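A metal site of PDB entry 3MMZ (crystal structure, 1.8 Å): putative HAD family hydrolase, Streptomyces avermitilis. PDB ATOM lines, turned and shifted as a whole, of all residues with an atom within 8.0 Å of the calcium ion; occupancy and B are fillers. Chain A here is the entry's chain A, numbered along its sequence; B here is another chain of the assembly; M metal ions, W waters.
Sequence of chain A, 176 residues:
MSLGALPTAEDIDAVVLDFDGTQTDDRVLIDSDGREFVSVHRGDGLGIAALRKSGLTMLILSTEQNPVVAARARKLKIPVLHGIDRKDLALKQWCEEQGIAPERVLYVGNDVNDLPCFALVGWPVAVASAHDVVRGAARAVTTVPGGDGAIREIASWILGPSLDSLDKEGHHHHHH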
ATOM      1  N   LEU A   3      28.999  26.097 -11.665  1.00  0.00           N
ATOM      2  CA  LEU A   3      28.419  24.827 -11.226  1.00  0.00           C
ATOM      3  C   LEU A   3      27.263  25.049 -10.249  1.00  0.00           C
ATOM      4  O   LEU A   3      27.380  25.808  -9.298  1.00  0.00           O
ATOM      5  CB  LEU A   3      29.494  23.951 -10.582  1.00  0.00           C
ATOM      6  CG  LEU A   3      29.061  22.576 -10.080  1.00  0.00           C
ATOM      7  CD1 LEU A   3      28.476  21.702 -11.195  1.00  0.00           C
ATOM      8  CD2 LEU A   3      30.227  21.879  -9.378  1.00  0.00           C
ATOM      9  N   GLY A   4      26.144  24.390 -10.511  1.00  0.00           N
ATOM     10  CA  GLY A   4      24.958  24.477  -9.649  1.00  0.00           C
ATOM     11  C   GLY A   4      24.084  25.709  -9.838  1.00  0.00           C
ATOM     12  O   GLY A   4      23.034  25.799  -9.200  1.00  0.00           O
ATOM     13  N   PRO A 124      17.459  19.825 -16.693  1.00  0.00           N
ATOM     14  CA  PRO A 124      16.525  18.956 -15.967  1.00  0.00           C
ATOM     15  C   PRO A 124      16.347  19.466 -14.551  1.00  0.00           C
ATOM     16  O   PRO A 124      17.336  19.807 -13.891  1.00  0.00           O
ATOM     17  CB  PRO A 124      17.245  17.611 -15.950  1.00  0.00           C
ATOM     18  CG  PRO A 124      18.694  17.940 -16.057  1.00  0.00           C
ATOM     19  CD  PRO A 124      18.759  19.160 -16.923  1.00  0.00           C
ATOM     20  N   VAL A 133      17.075   9.194  -6.913  1.00  0.00           N
ATOM     21  CA  VAL A 133      17.894   9.218  -8.117  1.00  0.00           C
ATOM     22  C   VAL A 133      17.534  10.403  -9.004  1.00  0.00           C
ATOM     23  O   VAL A 133      18.381  10.920  -9.741  1.00  0.00           O
ATOM     24  CB  VAL A 133      17.866   7.874  -8.911  1.00  0.00           C
ATOM     25  CG1 VAL A 133      18.575   6.781  -8.112  1.00  0.00           C
ATOM     26  CG2 VAL A 133      16.446   7.470  -9.251  1.00  0.00           C
ATOM     27  N   VAL A 134      16.271  10.824  -8.932  1.00  0.00           N
ATOM     28  CA  VAL A 134      15.788  11.928  -9.761  1.00  0.00           C
ATOM     29  C   VAL A 134      16.291  13.261  -9.212  1.00  0.00           C
ATOM     30  O   VAL A 134      16.685  14.141 -10.002  1.00  0.00           O
ATOM     31  CB  VAL A 134      14.251  11.917  -9.871  1.00  0.00           C
ATOM     32  CG1 VAL A 134      13.748  13.117 -10.693  1.00  0.00           C
ATOM     33  CG2 VAL A 134      13.786  10.594 -10.486  1.00  0.00           C
ATOM     34  N   ARG A 135      16.289  13.416  -7.882  1.00  0.00           N
ATOM     35  CA  ARG A 135      16.848  14.635  -7.249  1.00  0.00           C
ATOM     36  C   ARG A 135      18.320  14.808  -7.648  1.00  0.00           C
ATOM     37  O   ARG A 135      18.766  15.926  -7.949  1.00  0.00           O
ATOM     38  CB  ARG A 135      16.737  14.595  -5.705  1.00  0.00           C
ATOM     39  CG  ARG A 135      15.321  14.443  -5.185  1.00  0.00           C
ATOM     40  CD  ARG A 135      15.033  15.204  -3.861  1.00  0.00           C
ATOM     41  NE  ARG A 135      15.967  14.944  -2.757  1.00  0.00           N
ATOM     42  CZ  ARG A 135      15.883  15.563  -1.566  1.00  0.00           C
ATOM     43  NH1 ARG A 135      14.906  16.445  -1.352  1.00  0.00           N
ATOM     44  NH2 ARG A 135      16.761  15.302  -0.588  1.00  0.00           N
ATOM     45  N   GLY A 136      19.060  13.703  -7.625  1.00  0.00           N
ATOM     46  CA  GLY A 136      20.480  13.722  -7.991  1.00  0.00           C
ATOM     47  C   GLY A 136      20.692  14.046  -9.463  1.00  0.00           C
ATOM     48  O   GLY A 136      21.545  14.864  -9.796  1.00  0.00           O
ATOM     49  N   ALA A 137      19.933  13.375 -10.333  1.00  0.00           N
ATOM     50  CA  ALA A 137      20.074  13.526 -11.808  1.00  0.00           C
ATOM     51  C   ALA A 137      19.777  14.942 -12.301  1.00  0.00           C
ATOM     52  O   ALA A 137      20.278  15.357 -13.360  1.00  0.00           O
ATOM     53  CB  ALA A 137      19.162  12.550 -12.531  1.00  0.00           C
ATOM     54  N   ALA A 138      18.968  15.675 -11.550  1.00  0.00           N
ATOM     55  CA  ALA A 138      18.608  17.046 -11.920  1.00  0.00           C
ATOM     56  C   ALA A 138      19.787  18.013 -11.882  1.00  0.00           C
ATOM     57  O   ALA A 138      20.749  17.817 -11.138  1.00  0.00           O
ATOM     58  CB  ALA A 138      17.484  17.569 -11.014  1.00  0.00           C
ATOM     59  N   ARG A 139      19.666  19.105 -12.647  1.00  0.00           N
ATOM     60  CA  ARG A 139      20.640  20.185 -12.616  1.00  0.00           C
ATOM     61  C   ARG A 139      20.257  21.205 -11.536  1.00  0.00           C
ATOM     62  O   ARG A 139      21.114  21.928 -11.017  1.00  0.00           O
ATOM     63  CB  ARG A 139      20.699  20.878 -13.986  1.00  0.00           C
ATOM     64  CG  ARG A 139      21.771  21.950 -14.113  1.00  0.00           C
ATOM     65  CD  ARG A 139      21.913  22.364 -15.578  1.00  0.00           C
ATOM     66  NE  ARG A 139      22.898  23.427 -15.788  1.00  0.00           N
ATOM     67  CZ  ARG A 139      23.241  23.905 -16.985  1.00  0.00           C
ATOM     68  NH1 ARG A 139      22.688  23.406 -18.089  1.00  0.00           N
ATOM     69  NH2 ARG A 139      24.136  24.877 -17.092  1.00  0.00           N
ATOM     70  N   ALA A 140      18.958  21.257 -11.227  1.00  0.00           N
ATOM     71  CA  ALA A 140      18.453  22.071 -10.128  1.00  0.00           C
ATOM     72  C   ALA A 140      17.289  21.342  -9.465  1.00  0.00           C
ATOM     73  O   ALA A 140      16.620  20.522 -10.105  1.00  0.00           O
ATOM     74  CB  ALA A 140      18.022  23.429 -10.634  1.00  0.00           C
ATOM     75  N   VAL A 141      17.079  21.628  -8.190  1.00  0.00           N
ATOM     76  CA  VAL A 141      16.027  20.988  -7.410  1.00  0.00           C
ATOM     77  C   VAL A 141      15.222  22.066  -6.687  1.00  0.00           C
ATOM     78  O   VAL A 141      15.797  22.920  -6.016  1.00  0.00           O
ATOM     79  CB  VAL A 141      16.608  19.961  -6.363  1.00  0.00           C
ATOM     80  CG1 VAL A 141      15.484  19.180  -5.691  1.00  0.00           C
ATOM     81  CG2 VAL A 141      17.607  18.987  -7.012  1.00  0.00           C
ATOM     82  N   LEU B   3      21.866   7.402 -15.648  1.00  0.00           N
ATOM     83  CA  LEU B   3      21.692   8.730 -15.098  1.00  0.00           C
ATOM     84  C   LEU B   3      21.036   8.673 -13.721  1.00  0.00           C
ATOM     85  O   LEU B   3      20.016   8.016 -13.552  1.00  0.00           O
ATOM     86  CB  LEU B   3      20.872   9.599 -16.051  1.00  0.00           C
ATOM     87  CG  LEU B   3      20.552  11.038 -15.618  1.00  0.00           C
ATOM     88  CD1 LEU B   3      21.827  11.871 -15.444  1.00  0.00           C
ATOM     89  CD2 LEU B   3      19.595  11.680 -16.625  1.00  0.00           C
ATOM     90  N   GLY B   4      21.655   9.348 -12.754  1.00  0.00           N
ATOM     91  CA  GLY B   4      21.076   9.478 -11.400  1.00  0.00           C
ATOM     92  C   GLY B   4      21.406   8.315 -10.478  1.00  0.00           C
ATOM     93  O   GLY B   4      21.100   8.387  -9.281  1.00  0.00           O
ATOM     94  N   PHE B 118      33.292  19.732  -5.507  1.00  0.00           N
ATOM     95  CA  PHE B 118      32.289  19.032  -6.303  1.00  0.00           C
ATOM     96  C   PHE B 118      32.765  18.882  -7.750  1.00  0.00           C
ATOM     97  O   PHE B 118      32.686  17.800  -8.323  1.00  0.00           O
ATOM     98  CB  PHE B 118      30.942  19.788  -6.277  1.00  0.00           C
ATOM     99  CG  PHE B 118      30.016  19.398  -5.137  1.00  0.00           C
ATOM    100  CD1 PHE B 118      30.510  18.886  -3.941  1.00  0.00           C
ATOM    101  CD2 PHE B 118      28.634  19.579  -5.274  1.00  0.00           C
ATOM    102  CE1 PHE B 118      29.620  18.528  -2.903  1.00  0.00           C
ATOM    103  CE2 PHE B 118      27.757  19.236  -4.256  1.00  0.00           C
ATOM    104  CZ  PHE B 118      28.243  18.703  -3.061  1.00  0.00           C
ATOM    105  N   PRO B 124      30.232  13.841  -6.370  1.00  0.00           N
ATOM    106  CA  PRO B 124      29.882  14.839  -5.362  1.00  0.00           C
ATOM    107  C   PRO B 124      28.500  14.520  -4.801  1.00  0.00           C
ATOM    108  O   PRO B 124      27.600  14.194  -5.578  1.00  0.00           O
ATOM    109  CB  PRO B 124      29.840  16.147  -6.159  1.00  0.00           C
ATOM    110  CG  PRO B 124      29.598  15.739  -7.583  1.00  0.00           C
ATOM    111  CD  PRO B 124      30.259  14.412  -7.740  1.00  0.00           C
ATOM    112  N   VAL B 133      21.893  25.603  -4.479  1.00  0.00           N
ATOM    113  CA  VAL B 133      22.773  25.366  -5.640  1.00  0.00           C
ATOM    114  C   VAL B 133      23.637  24.120  -5.468  1.00  0.00           C
ATOM    115  O   VAL B 133      24.010  23.461  -6.446  1.00  0.00           O
ATOM    116  CB  VAL B 133      23.651  26.602  -5.995  1.00  0.00           C
ATOM    117  CG1 VAL B 133      22.783  27.829  -6.273  1.00  0.00           C
ATOM    118  CG2 VAL B 133      24.671  26.895  -4.905  1.00  0.00           C
ATOM    119  N   VAL B 134      23.937  23.777  -4.221  1.00  0.00           N
ATOM    120  CA  VAL B 134      24.751  22.610  -3.887  1.00  0.00           C
ATOM    121  C   VAL B 134      23.955  21.320  -4.118  1.00  0.00           C
ATOM    122  O   VAL B 134      24.473  20.350  -4.659  1.00  0.00           O
ATOM    123  CB  VAL B 134      25.277  22.699  -2.432  1.00  0.00           C
ATOM    124  CG1 VAL B 134      26.117  21.457  -2.066  1.00  0.00           C
ATOM    125  CG2 VAL B 134      26.110  23.966  -2.243  1.00  0.00           C
ATOM    126  N   ARG B 135      22.682  21.314  -3.714  1.00  0.00           N
ATOM    127  CA  ARG B 135      21.808  20.180  -3.993  1.00  0.00           C
ATOM    128  C   ARG B 135      21.741  19.900  -5.488  1.00  0.00           C
ATOM    129  O   ARG B 135      21.862  18.751  -5.925  1.00  0.00           O
ATOM    130  CB  ARG B 135      20.399  20.438  -3.454  1.00  0.00           C
ATOM    131  CG  ARG B 135      20.274  20.290  -1.967  1.00  0.00           C
ATOM    132  CD  ARG B 135      19.098  21.107  -1.468  1.00  0.00           C
ATOM    133  NE  ARG B 135      17.775  20.540  -1.702  1.00  0.00           N
ATOM    134  CZ  ARG B 135      16.810  21.114  -2.438  1.00  0.00           C
ATOM    135  NH1 ARG B 135      17.022  22.281  -3.056  1.00  0.00           N
ATOM    136  NH2 ARG B 135      15.611  20.514  -2.544  1.00  0.00           N
ATOM    137  N   GLY B 136      21.601  20.966  -6.273  1.00  0.00           N
ATOM    138  CA  GLY B 136      21.591  20.826  -7.739  1.00  0.00           C
ATOM    139  C   GLY B 136      22.889  20.276  -8.303  1.00  0.00           C
ATOM    140  O   GLY B 136      22.892  19.342  -9.110  1.00  0.00           O
ATOM    141  N   ALA B 137      24.012  20.858  -7.865  1.00  0.00           N
ATOM    142  CA  ALA B 137      25.354  20.520  -8.367  1.00  0.00           C
ATOM    143  C   ALA B 137      25.785  19.087  -8.092  1.00  0.00           C
ATOM    144  O   ALA B 137      26.596  18.528  -8.817  1.00  0.00           O
ATOM    145  CB  ALA B 137      26.380  21.501  -7.791  1.00  0.00           C
ATOM    146  N   ALA B 138      25.258  18.513  -7.016  1.00  0.00           N
ATOM    147  CA  ALA B 138      25.585  17.150  -6.622  1.00  0.00           C
ATOM    148  C   ALA B 138      25.159  16.112  -7.660  1.00  0.00           C
ATOM    149  O   ALA B 138      24.243  16.320  -8.464  1.00  0.00           O
ATOM    150  CB  ALA B 138      24.948  16.833  -5.279  1.00  0.00           C
ATOM    151  N   ARG B 139      25.847  14.971  -7.628  1.00  0.00           N
ATOM    152  CA  ARG B 139      25.477  13.828  -8.436  1.00  0.00           C
ATOM    153  C   ARG B 139      24.437  12.965  -7.707  1.00  0.00           C
ATOM    154  O   ARG B 139      23.636  12.270  -8.337  1.00  0.00           O
ATOM    155  CB  ARG B 139      26.732  13.011  -8.775  1.00  0.00           C
ATOM    156  CG  ARG B 139      26.526  11.860  -9.726  1.00  0.00           C
ATOM    157  CD  ARG B 139      27.856  11.282 -10.161  1.00  0.00           C
ATOM    158  NE  ARG B 139      27.684  10.104 -11.021  1.00  0.00           N
ATOM    159  CZ  ARG B 139      28.685   9.479 -11.647  1.00  0.00           C
ATOM    160  NH1 ARG B 139      29.944   9.897 -11.513  1.00  0.00           N
ATOM    161  NH2 ARG B 139      28.435   8.419 -12.397  1.00  0.00           N
ATOM    162  N   ALA B 140      24.437  13.056  -6.382  1.00  0.00           N
ATOM    163  CA  ALA B 140      23.466  12.369  -5.532  1.00  0.00           C
ATOM    164  C   ALA B 140      23.142  13.282  -4.342  1.00  0.00           C
ATOM    165  O   ALA B 140      23.980  14.106  -3.951  1.00  0.00           O
ATOM    166  CB  ALA B 140      24.030  11.043  -5.073  1.00  0.00           C
ATOM    167  N   VAL B 141      21.930  13.158  -3.794  1.00  0.00           N
ATOM    168  CA  VAL B 141      21.494  14.014  -2.679  1.00  0.00           C
ATOM    169  C   VAL B 141      20.896  13.105  -1.620  1.00  0.00           C
ATOM    170  O   VAL B 141      20.061  12.248  -1.943  1.00  0.00           O
ATOM    171  CB  VAL B 141      20.429  15.064  -3.143  1.00  0.00           C
ATOM    172  CG1 VAL B 141      19.994  15.973  -1.989  1.00  0.00           C
ATOM    173  CG2 VAL B 141      20.954  15.911  -4.323  1.00  0.00           C
HETATM  174 CA    CA M   1      22.553  17.067  -9.833  1.00  0.00          CA
HETATM  175  O   HOH W   1      24.032  18.208 -11.562  1.00  0.00           O
HETATM  176  O   HOH W   2      21.182  17.160  -7.947  1.00  0.00           O
HETATM  177  O   HOH W   3      23.553  15.540 -11.563  1.00  0.00           O
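Four residues have an atom within 4 Å of the calcium ion: Gly 136 of chain A, Ala 138 of chain A, Gly 136 of chain B and Ala 138 of chain B.
The nearest printed residue that does not touch the calcium ion is Ala 137 of chain B (4.2 Å).
Water W2 bridges O of Arg 135 of chain B (2.7 Å) and O of Arg 135 of chain A (2.7 Å).
The calcium ion is bound by the backbone carbonyl oxygen (O) of Ala 138 of chain B (2.3 Å), water W2 (2.3 Å), the backbone carbonyl oxygen (O) of Ala 138 of chain A (2.3 Å), the backbone carbonyl oxygen (O) of Gly 136 of chain B (2.4 Å), the backbone carbonyl oxygen (O) of Gly 136 of chain A (2.4 Å), water W3 (2.5 Å) and water W1 (2.5 Å).
The calcium ion has seven donor atoms within binding distance.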
